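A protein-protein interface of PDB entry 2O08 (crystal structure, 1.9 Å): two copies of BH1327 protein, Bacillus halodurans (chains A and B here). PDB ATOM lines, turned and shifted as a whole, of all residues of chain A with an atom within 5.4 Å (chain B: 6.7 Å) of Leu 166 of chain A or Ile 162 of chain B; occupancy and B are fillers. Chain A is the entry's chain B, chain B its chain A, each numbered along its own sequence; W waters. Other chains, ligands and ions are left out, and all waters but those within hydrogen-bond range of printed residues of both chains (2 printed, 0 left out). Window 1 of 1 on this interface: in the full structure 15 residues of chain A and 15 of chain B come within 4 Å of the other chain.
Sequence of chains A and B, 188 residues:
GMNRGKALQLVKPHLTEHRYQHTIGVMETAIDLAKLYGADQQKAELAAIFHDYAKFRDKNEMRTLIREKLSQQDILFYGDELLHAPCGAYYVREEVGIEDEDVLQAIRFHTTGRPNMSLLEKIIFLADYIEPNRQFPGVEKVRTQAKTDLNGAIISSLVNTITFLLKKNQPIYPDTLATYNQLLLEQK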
ATOM      1  N   THR A 161     -17.591  15.819 -21.026  1.00  0.00           N
ATOM      2  CA  THR A 161     -17.297  15.295 -22.361  1.00  0.00           C
ATOM      3  C   THR A 161     -15.819  15.444 -22.725  1.00  0.00           C
ATOM      4  O   THR A 161     -15.149  14.474 -23.079  1.00  0.00           O
ATOM      5  CB  THR A 161     -18.211  15.999 -23.403  1.00  0.00           C
ATOM      6  OG1 THR A 161     -19.579  15.706 -23.088  1.00  0.00           O
ATOM      7  CG2 THR A 161     -17.885  15.588 -24.841  1.00  0.00           C
ATOM      8  N   ILE A 162     -15.293  16.660 -22.592  1.00  0.00           N
ATOM      9  CA  ILE A 162     -13.910  16.927 -22.965  1.00  0.00           C
ATOM     10  C   ILE A 162     -12.969  16.101 -22.066  1.00  0.00           C
ATOM     11  O   ILE A 162     -11.993  15.516 -22.555  1.00  0.00           O
ATOM     12  CB  ILE A 162     -13.563  18.429 -22.962  1.00  0.00           C
ATOM     13  CG1 ILE A 162     -14.453  19.173 -23.981  1.00  0.00           C
ATOM     14  CG2 ILE A 162     -12.071  18.615 -23.360  1.00  0.00           C
ATOM     15  CD1 ILE A 162     -14.354  20.717 -23.939  1.00  0.00           C
ATOM     16  N   THR A 163     -13.308  16.007 -20.783  1.00  0.00           N
ATOM     17  CA  THR A 163     -12.521  15.211 -19.843  1.00  0.00           C
ATOM     18  C   THR A 163     -12.450  13.765 -20.286  1.00  0.00           C
ATOM     19  O   THR A 163     -11.377  13.175 -20.329  1.00  0.00           O
ATOM     20  CB  THR A 163     -13.070  15.296 -18.398  1.00  0.00           C
ATOM     21  OG1 THR A 163     -12.805  16.602 -17.878  1.00  0.00           O
ATOM     22  CG2 THR A 163     -12.367  14.271 -17.481  1.00  0.00           C
ATOM     23  N   PHE A 164     -13.602  13.229 -20.675  1.00  0.00           N
ATOM     24  CA  PHE A 164     -13.699  11.849 -21.129  1.00  0.00           C
ATOM     25  C   PHE A 164     -12.842  11.616 -22.359  1.00  0.00           C
ATOM     26  O   PHE A 164     -12.060  10.663 -22.391  1.00  0.00           O
ATOM     27  CB  PHE A 164     -15.172  11.526 -21.384  1.00  0.00           C
ATOM     28  CG  PHE A 164     -15.392  10.165 -21.925  1.00  0.00           C
ATOM     29  CD1 PHE A 164     -15.545   9.097 -21.067  1.00  0.00           C
ATOM     30  CD2 PHE A 164     -15.387   9.937 -23.309  1.00  0.00           C
ATOM     31  CE1 PHE A 164     -15.746   7.814 -21.585  1.00  0.00           C
ATOM     32  CE2 PHE A 164     -15.560   8.653 -23.825  1.00  0.00           C
ATOM     33  CZ  PHE A 164     -15.743   7.601 -22.969  1.00  0.00           C
ATOM     34  N   LEU A 165     -12.961  12.496 -23.368  1.00  0.00           N
ATOM     35  CA  LEU A 165     -12.140  12.379 -24.599  1.00  0.00           C
ATOM     36  C   LEU A 165     -10.629  12.397 -24.284  1.00  0.00           C
ATOM     37  O   LEU A 165      -9.866  11.572 -24.783  1.00  0.00           O
ATOM     38  CB  LEU A 165     -12.530  13.484 -25.620  1.00  0.00           C
ATOM     39  CG  LEU A 165     -13.961  13.409 -26.206  1.00  0.00           C
ATOM     40  CD1 LEU A 165     -14.462  14.752 -26.862  1.00  0.00           C
ATOM     41  CD2 LEU A 165     -14.033  12.180 -27.212  1.00  0.00           C
ATOM     42  N   LEU A 166     -10.200  13.339 -23.443  1.00  0.00           N
ATOM     43  CA  LEU A 166      -8.792  13.390 -22.994  1.00  0.00           C
ATOM     44  C   LEU A 166      -8.338  12.097 -22.337  1.00  0.00           C
ATOM     45  O   LEU A 166      -7.291  11.557 -22.722  1.00  0.00           O
ATOM     46  CB  LEU A 166      -8.519  14.565 -22.033  1.00  0.00           C
ATOM     47  CG  LEU A 166      -8.649  15.968 -22.636  1.00  0.00           C
ATOM     48  CD1 LEU A 166      -8.741  17.003 -21.533  1.00  0.00           C
ATOM     49  CD2 LEU A 166      -7.516  16.299 -23.581  1.00  0.00           C
ATOM     50  N   LYS A 167      -9.129  11.580 -21.388  1.00  0.00           N
ATOM     51  CA  LYS A 167      -8.794  10.334 -20.709  1.00  0.00           C
ATOM     52  C   LYS A 167      -8.659   9.236 -21.748  1.00  0.00           C
ATOM     53  O   LYS A 167      -7.741   8.449 -21.669  1.00  0.00           O
ATOM     54  CB  LYS A 167      -9.832   9.883 -19.675  1.00  0.00           C
ATOM     55  CG  LYS A 167      -9.615  10.446 -18.286  1.00  0.00           C
ATOM     56  N   LYS A 168      -9.562   9.196 -22.714  1.00  0.00           N
ATOM     57  CA  LYS A 168      -9.470   8.187 -23.772  1.00  0.00           C
ATOM     58  C   LYS A 168      -8.434   8.504 -24.866  1.00  0.00           C
ATOM     59  O   LYS A 168      -8.279   7.720 -25.802  1.00  0.00           O
ATOM     60  CB  LYS A 168     -10.844   7.969 -24.414  1.00  0.00           C
ATOM     61  CG  LYS A 168     -11.915   7.350 -23.511  1.00  0.00           C
ATOM     62  CD  LYS A 168     -11.481   5.964 -23.042  1.00  0.00           C
ATOM     63  CE  LYS A 168     -12.605   5.131 -22.485  1.00  0.00           C
ATOM     64  NZ  LYS A 168     -13.363   5.869 -21.479  1.00  0.00           N
ATOM     65  N   ASN A 169      -7.725   9.622 -24.760  1.00  0.00           N
ATOM     66  CA  ASN A 169      -6.744  10.050 -25.753  1.00  0.00           C
ATOM     67  C   ASN A 169      -7.354  10.063 -27.125  1.00  0.00           C
ATOM     68  O   ASN A 169      -6.808   9.509 -28.054  1.00  0.00           O
ATOM     69  CB  ASN A 169      -5.455   9.197 -25.729  1.00  0.00           C
ATOM     70  CG  ASN A 169      -4.549   9.518 -24.536  1.00  0.00           C
ATOM     71  OD1 ASN A 169      -4.898  10.271 -23.619  1.00  0.00           O
ATOM     72  ND2 ASN A 169      -3.381   8.930 -24.554  1.00  0.00           N
ATOM     73  N   GLN A 170      -8.524  10.687 -27.224  1.00  0.00           N
ATOM     74  CA  GLN A 170      -9.222  10.862 -28.489  1.00  0.00           C
ATOM     75  C   GLN A 170      -9.101  12.367 -28.852  1.00  0.00           C
ATOM     76  O   GLN A 170      -8.899  13.200 -27.970  1.00  0.00           O
ATOM     77  CB  GLN A 170     -10.676  10.381 -28.339  1.00  0.00           C
ATOM     78  CG  GLN A 170     -10.788   8.825 -28.198  1.00  0.00           C
ATOM     79  CD  GLN A 170     -12.204   8.317 -27.813  1.00  0.00           C
ATOM     80  OE1 GLN A 170     -13.135   9.106 -27.621  1.00  0.00           O
ATOM     81  NE2 GLN A 170     -12.359   6.988 -27.710  1.00  0.00           N
ATOM     82  N   ILE A 172     -10.165  16.158 -29.892  1.00  0.00           N
ATOM     83  CA  ILE A 172     -11.246  17.001 -29.416  1.00  0.00           C
ATOM     84  C   ILE A 172     -11.450  18.120 -30.442  1.00  0.00           C
ATOM     85  O   ILE A 172     -10.560  18.928 -30.705  1.00  0.00           O
ATOM     86  CB  ILE A 172     -10.893  17.548 -28.015  1.00  0.00           C
ATOM     87  CG1 ILE A 172     -10.744  16.360 -27.034  1.00  0.00           C
ATOM     88  CG2 ILE A 172     -11.967  18.535 -27.543  1.00  0.00           C
ATOM     89  CD1 ILE A 172      -9.952  16.676 -25.803  1.00  0.00           C
ATOM     90  N   ILE B 155       1.827  14.479 -24.472  1.00  0.00           N
ATOM     91  CA  ILE B 155       0.363  14.263 -24.528  1.00  0.00           C
ATOM     92  C   ILE B 155      -0.237  14.047 -23.117  1.00  0.00           C
ATOM     93  O   ILE B 155      -1.206  14.697 -22.718  1.00  0.00           O
ATOM     94  CB  ILE B 155       0.007  13.080 -25.441  1.00  0.00           C
ATOM     95  CG1 ILE B 155       0.215  13.473 -26.913  1.00  0.00           C
ATOM     96  CG2 ILE B 155      -1.426  12.658 -25.196  1.00  0.00           C
ATOM     97  CD1 ILE B 155       0.312  12.293 -27.917  1.00  0.00           C
ATOM     98  N   SER B 157       0.943  15.006 -20.285  1.00  0.00           N
ATOM     99  CA  SER B 157       1.019  16.218 -19.491  1.00  0.00           C
ATOM    100  C   SER B 157      -0.132  17.171 -19.831  1.00  0.00           C
ATOM    101  O   SER B 157      -0.723  17.760 -18.948  1.00  0.00           O
ATOM    102  CB  SER B 157       2.341  16.933 -19.718  1.00  0.00           C
ATOM    103  OG  SER B 157       2.424  17.418 -21.050  1.00  0.00           O
ATOM    104  N   LEU B 158      -0.394  17.341 -21.129  1.00  0.00           N
ATOM    105  CA  LEU B 158      -1.489  18.163 -21.639  1.00  0.00           C
ATOM    106  C   LEU B 158      -2.843  17.640 -21.158  1.00  0.00           C
ATOM    107  O   LEU B 158      -3.712  18.426 -20.761  1.00  0.00           O
ATOM    108  CB  LEU B 158      -1.409  18.241 -23.176  1.00  0.00           C
ATOM    109  CG  LEU B 158      -0.249  19.059 -23.760  1.00  0.00           C
ATOM    110  CD1 LEU B 158       0.028  18.788 -25.253  1.00  0.00           C
ATOM    111  CD2 LEU B 158      -0.495  20.538 -23.540  1.00  0.00           C
ATOM    112  N   VAL B 159      -3.024  16.318 -21.195  1.00  0.00           N
ATOM    113  CA  VAL B 159      -4.232  15.673 -20.681  1.00  0.00           C
ATOM    114  C   VAL B 159      -4.452  16.101 -19.214  1.00  0.00           C
ATOM    115  O   VAL B 159      -5.527  16.599 -18.865  1.00  0.00           O
ATOM    116  CB  VAL B 159      -4.183  14.137 -20.855  1.00  0.00           C
ATOM    117  CG1 VAL B 159      -5.246  13.418 -19.988  1.00  0.00           C
ATOM    118  CG2 VAL B 159      -4.372  13.783 -22.350  1.00  0.00           C
ATOM    119  N   ASN B 160      -3.426  15.959 -18.377  1.00  0.00           N
ATOM    120  CA  ASN B 160      -3.567  16.315 -16.973  1.00  0.00           C
ATOM    121  C   ASN B 160      -3.804  17.843 -16.805  1.00  0.00           C
ATOM    122  O   ASN B 160      -4.637  18.250 -15.987  1.00  0.00           O
ATOM    123  CB  ASN B 160      -2.376  15.756 -16.156  1.00  0.00           C
ATOM    124  CG  ASN B 160      -2.291  14.208 -16.186  1.00  0.00           C
ATOM    125  OD1 ASN B 160      -3.197  13.519 -16.674  1.00  0.00           O
ATOM    126  ND2 ASN B 160      -1.191  13.667 -15.667  1.00  0.00           N
ATOM    127  N   THR B 161      -3.111  18.663 -17.596  1.00  0.00           N
ATOM    128  CA  THR B 161      -3.289  20.112 -17.540  1.00  0.00           C
ATOM    129  C   THR B 161      -4.694  20.548 -17.940  1.00  0.00           C
ATOM    130  O   THR B 161      -5.379  21.246 -17.189  1.00  0.00           O
ATOM    131  CB  THR B 161      -2.256  20.861 -18.420  1.00  0.00           C
ATOM    132  OG1 THR B 161      -0.972  20.734 -17.812  1.00  0.00           O
ATOM    133  CG2 THR B 161      -2.603  22.360 -18.548  1.00  0.00           C
ATOM    134  N   ILE B 162      -5.109  20.110 -19.118  1.00  0.00           N
ATOM    135  CA  ILE B 162      -6.412  20.487 -19.649  1.00  0.00           C
ATOM    136  C   ILE B 162      -7.498  19.925 -18.740  1.00  0.00           C
ATOM    137  O   ILE B 162      -8.452  20.618 -18.452  1.00  0.00           O
ATOM    138  CB  ILE B 162      -6.608  20.042 -21.126  1.00  0.00           C
ATOM    139  CG1 ILE B 162      -5.568  20.730 -22.030  1.00  0.00           C
ATOM    140  CG2 ILE B 162      -8.037  20.380 -21.582  1.00  0.00           C
ATOM    141  CD1 ILE B 162      -5.388  20.110 -23.449  1.00  0.00           C
ATOM    142  N   THR B 163      -7.331  18.692 -18.252  1.00  0.00           N
ATOM    143  CA  THR B 163      -8.331  18.120 -17.353  1.00  0.00           C
ATOM    144  C   THR B 163      -8.528  18.978 -16.112  1.00  0.00           C
ATOM    145  O   THR B 163      -9.653  19.208 -15.690  1.00  0.00           O
ATOM    146  CB  THR B 163      -7.963  16.682 -16.967  1.00  0.00           C
ATOM    147  OG1 THR B 163      -8.092  15.855 -18.133  1.00  0.00           O
ATOM    148  CG2 THR B 163      -8.885  16.126 -15.868  1.00  0.00           C
ATOM    149  N   PHE B 164      -7.418  19.440 -15.539  1.00  0.00           N
ATOM    150  CA  PHE B 164      -7.421  20.249 -14.329  1.00  0.00           C
ATOM    151  C   PHE B 164      -8.110  21.568 -14.571  1.00  0.00           C
ATOM    152  O   PHE B 164      -8.953  21.981 -13.793  1.00  0.00           O
ATOM    153  CB  PHE B 164      -5.986  20.508 -13.862  1.00  0.00           C
ATOM    154  CG  PHE B 164      -5.902  21.382 -12.656  1.00  0.00           C
ATOM    155  CD1 PHE B 164      -6.134  20.848 -11.393  1.00  0.00           C
ATOM    156  CD2 PHE B 164      -5.647  22.750 -12.783  1.00  0.00           C
ATOM    157  CE1 PHE B 164      -6.094  21.660 -10.264  1.00  0.00           C
ATOM    158  CE2 PHE B 164      -5.603  23.576 -11.647  1.00  0.00           C
ATOM    159  CZ  PHE B 164      -5.834  23.017 -10.389  1.00  0.00           C
ATOM    160  N   LEU B 165      -7.749  22.234 -15.653  1.00  0.00           N
ATOM    161  CA  LEU B 165      -8.368  23.513 -15.982  1.00  0.00           C
ATOM    162  C   LEU B 165      -9.905  23.372 -16.183  1.00  0.00           C
ATOM    163  O   LEU B 165     -10.685  24.257 -15.773  1.00  0.00           O
ATOM    164  CB  LEU B 165      -7.682  24.130 -17.232  1.00  0.00           C
ATOM    165  CG  LEU B 165      -6.207  24.594 -17.123  1.00  0.00           C
ATOM    166  CD1 LEU B 165      -5.703  25.052 -18.466  1.00  0.00           C
ATOM    167  CD2 LEU B 165      -6.061  25.712 -16.086  1.00  0.00           C
ATOM    168  N   LEU B 166     -10.329  22.283 -16.838  1.00  0.00           N
ATOM    169  CA  LEU B 166     -11.758  22.024 -17.063  1.00  0.00           C
ATOM    170  C   LEU B 166     -12.491  21.857 -15.753  1.00  0.00           C
ATOM    171  O   LEU B 166     -13.551  22.457 -15.542  1.00  0.00           O
ATOM    172  CB  LEU B 166     -11.961  20.773 -17.940  1.00  0.00           C
ATOM    173  CG  LEU B 166     -11.669  20.955 -19.431  1.00  0.00           C
ATOM    174  CD1 LEU B 166     -11.612  19.565 -20.078  1.00  0.00           C
ATOM    175  CD2 LEU B 166     -12.720  21.859 -20.133  1.00  0.00           C
ATOM    176  N   LYS B 167     -11.882  21.078 -14.858  1.00  0.00           N
ATOM    177  CA  LYS B 167     -12.418  20.769 -13.518  1.00  0.00           C
ATOM    178  C   LYS B 167     -12.551  22.005 -12.653  1.00  0.00           C
ATOM    179  O   LYS B 167     -13.490  22.111 -11.893  1.00  0.00           O
ATOM    180  CB  LYS B 167     -11.473  19.784 -12.825  1.00  0.00           C
ATOM    181  CG  LYS B 167     -11.832  19.369 -11.412  1.00  0.00           C
ATOM    182  N   ILE B 172      -9.392  27.712 -21.350  1.00  0.00           N
ATOM    183  CA  ILE B 172      -8.298  26.928 -21.920  1.00  0.00           C
ATOM    184  C   ILE B 172      -7.859  27.566 -23.239  1.00  0.00           C
ATOM    185  O   ILE B 172      -8.654  27.818 -24.127  1.00  0.00           O
ATOM    186  CB  ILE B 172      -8.714  25.463 -22.062  1.00  0.00           C
ATOM    187  CG1 ILE B 172      -8.984  24.888 -20.671  1.00  0.00           C
ATOM    188  CG2 ILE B 172      -7.643  24.647 -22.842  1.00  0.00           C
ATOM    189  CD1 ILE B 172      -9.949  23.720 -20.691  1.00  0.00           C
ATOM    190  N   TYR B 173      -6.566  27.851 -23.322  1.00  0.00           N
ATOM    191  CA  TYR B 173      -5.951  28.465 -24.477  1.00  0.00           C
ATOM    192  C   TYR B 173      -6.100  27.494 -25.627  1.00  0.00           C
ATOM    193  O   TYR B 173      -5.671  26.350 -25.529  1.00  0.00           O
ATOM    194  CB  TYR B 173      -4.490  28.780 -24.204  1.00  0.00           C
ATOM    195  CG  TYR B 173      -3.821  29.622 -25.264  1.00  0.00           C
ATOM    196  CD1 TYR B 173      -4.297  30.906 -25.575  1.00  0.00           C
ATOM    197  CD2 TYR B 173      -2.720  29.143 -25.958  1.00  0.00           C
ATOM    198  CE1 TYR B 173      -3.667  31.693 -26.542  1.00  0.00           C
ATOM    199  CE2 TYR B 173      -2.095  29.910 -26.914  1.00  0.00           C
ATOM    200  CZ  TYR B 173      -2.565  31.183 -27.208  1.00  0.00           C
ATOM    201  OH  TYR B 173      -1.920  31.903 -28.190  1.00  0.00           O
ATOM    202  N   THR B 176      -3.216  25.322 -27.017  1.00  0.00           N
ATOM    203  CA  THR B 176      -2.822  24.208 -26.147  1.00  0.00           C
ATOM    204  C   THR B 176      -3.560  22.921 -26.536  1.00  0.00           C
ATOM    205  O   THR B 176      -2.960  21.830 -26.588  1.00  0.00           O
ATOM    206  CB  THR B 176      -3.066  24.577 -24.696  1.00  0.00           C
ATOM    207  OG1 THR B 176      -2.194  25.666 -24.398  1.00  0.00           O
ATOM    208  CG2 THR B 176      -2.783  23.374 -23.729  1.00  0.00           C
ATOM    209  N   LEU B 177      -4.843  23.052 -26.835  1.00  0.00           N
ATOM    210  CA  LEU B 177      -5.607  21.934 -27.364  1.00  0.00           C
ATOM    211  C   LEU B 177      -5.116  21.568 -28.759  1.00  0.00           C
ATOM    212  O   LEU B 177      -5.055  20.408 -29.102  1.00  0.00           O
ATOM    213  CB  LEU B 177      -7.109  22.278 -27.406  1.00  0.00           C
ATOM    214  CG  LEU B 177      -8.010  21.087 -27.804  1.00  0.00           C
ATOM    215  CD1 LEU B 177      -8.007  20.031 -26.731  1.00  0.00           C
ATOM    216  CD2 LEU B 177      -9.422  21.549 -28.096  1.00  0.00           C
ATOM    217  N   ALA B 178      -4.779  22.555 -29.585  1.00  0.00           N
ATOM    218  CA  ALA B 178      -4.266  22.260 -30.915  1.00  0.00           C
ATOM    219  C   ALA B 178      -2.995  21.450 -30.774  1.00  0.00           C
ATOM    220  O   ALA B 178      -2.759  20.554 -31.566  1.00  0.00           O
ATOM    221  CB  ALA B 178      -4.016  23.519 -31.716  1.00  0.00           C
ATOM    222  N   TYR B 180      -2.185  19.312 -28.235  1.00  0.00           N
ATOM    223  CA  TYR B 180      -2.666  17.974 -27.917  1.00  0.00           C
ATOM    224  C   TYR B 180      -3.140  17.243 -29.146  1.00  0.00           C
ATOM    225  O   TYR B 180      -2.716  16.121 -29.412  1.00  0.00           O
ATOM    226  CB  TYR B 180      -3.821  18.082 -26.930  1.00  0.00           C
ATOM    227  CG  TYR B 180      -4.623  16.836 -26.763  1.00  0.00           C
ATOM    228  CD1 TYR B 180      -4.186  15.814 -25.923  1.00  0.00           C
ATOM    229  CD2 TYR B 180      -5.830  16.667 -27.445  1.00  0.00           C
ATOM    230  CE1 TYR B 180      -4.919  14.658 -25.769  1.00  0.00           C
ATOM    231  CE2 TYR B 180      -6.581  15.528 -27.288  1.00  0.00           C
ATOM    232  CZ  TYR B 180      -6.130  14.512 -26.458  1.00  0.00           C
ATOM    233  OH  TYR B 180      -6.881  13.370 -26.323  1.00  0.00           O
ATOM    234  N   LEU B 184      -1.382  14.067 -30.820  1.00  0.00           N
ATOM    235  CA  LEU B 184      -2.245  12.906 -30.810  1.00  0.00           C
ATOM    236  C   LEU B 184      -2.369  12.365 -32.221  1.00  0.00           C
ATOM    237  O   LEU B 184      -2.045  11.213 -32.459  1.00  0.00           O
ATOM    238  CB  LEU B 184      -3.634  13.269 -30.281  1.00  0.00           C
ATOM    239  CG  LEU B 184      -4.508  12.107 -29.851  1.00  0.00           C
ATOM    240  CD1 LEU B 184      -4.038  11.549 -28.486  1.00  0.00           C
ATOM    241  CD2 LEU B 184      -5.963  12.582 -29.811  1.00  0.00           C
HETATM  242  O   HOH W   1     -11.834  17.611 -15.675  1.00  0.00           O
HETATM  243  O   HOH W   2      -9.126  13.322 -18.490  1.00  0.00           O
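Among the printed residues, pairs that only touch across the chains: Gln 170 of chain A with Leu 184 of chain B (3.3 Å), Asn 169 of chain A with Tyr 180 of chain B (3.4 Å), Ile 162 of chain A with Leu 166 of chain B (3.4 Å), Leu 166 of chain A with Ile 162 of chain B (3.4 Å), Asn 169 of chain A with Leu 184 of chain B (3.5 Å), Leu 166 of chain A with Thr 163 of chain B (3.6 Å), Leu 166 of chain A with Tyr 180 of chain B (3.7 Å), Leu 166 of chain A with Val 159 of chain B (3.7 Å), Asn 169 of chain A with Val 159 of chain B (3.8 Å), Leu 165 of chain A with Tyr 180 of chain B (3.8 Å), Ile 172 of chain A with Tyr 180 of chain B (3.9 Å), Ile 172 of chain A with Leu 177 of chain B (3.9 Å) and Thr 163 of chain A with Leu 166 of chain B (3.9 Å).
Along chain A the printed residues that touch a printed residue of chain B span positions 162 to 172.
Hydrophobic or aromatic side chains of chain B within 4 Å of the printed part of chain A: Val 159, Ile 162, Leu 166, Leu 177, Tyr 180 and Leu 184.
Along chain B the printed residues that touch a printed residue of chain A span positions 159 to 184.
Water W1 bridges OG1 of Thr 163 of chain A (2.6 Å) and O of Thr 163 of chain B (2.7 Å).
Water W2 lies within hydrogen-bond range of the side-chain hydroxyl of Thr 163 of chain B, the backbone carbonyl oxygen of Thr 163 of chain A and the backbone NH of Lys 167 of chain A.
OH of Tyr 180 of chain B sits at hydrogen-bond distance from O of Gln 170 of chain A, 2.6 Å away.
Ile 162 of chain A touches Leu 166 of chain B, and with the chains exchanged Leu 166 of chain A touches Ile 162 of chain B.
Thr 163 of chain A touches Leu 166 of chain B, and with the chains exchanged Leu 166 of chain A touches Thr 163 of chain B.
Positions printed for both chains: 161, 162, 163, 164, 165, 166, 167 and 172.
N of Gln 170 of chain A sits at hydrogen-bond distance from O of Leu 165 of chain A (2.9 Å).
The backbone carbonyl oxygen (O) of Leu 166 of chain A lies close to the side-chain amide oxygen (OD1) of Asn 169 of chain A (2.9 Å).
OG1 of Thr 163 of chain B lies within hydrogen-bond range of O of Val 159 of chain B (2.8 Å).
Printed residues of chain B within 4 Å of Ile 162 of chain A: Leu 166.
Of the printed residues of chain B, Leu 165 of chain A touches Tyr 180 (3.8 Å).
Leu 166 of chain A touches four residues of chain B.
Lys 168 of chain A touches none of the printed residues of chain B.
Printed residues of chain B within 4 Å of Gln 170 of chain A: Tyr 180 (2.6 Å) and Leu 184 (3.3 Å).
Ile 162 of chain B touches just one residue of chain A: Leu 166 (3.4 Å).
Leu 165 of chain B touches none of the printed residues of chain A.
Of the printed residues of chain A, Tyr 180 of chain B touches Leu 165 (3.8 Å), Leu 166 (3.7 Å), Asn 169 (3.4 Å), Gln 170 (2.6 Å) and Ile 172 (3.9 Å).
The nearest residue of chain A that does not touch Ile 162 of chain B is Ile 162 of chain A (4.7 Å).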
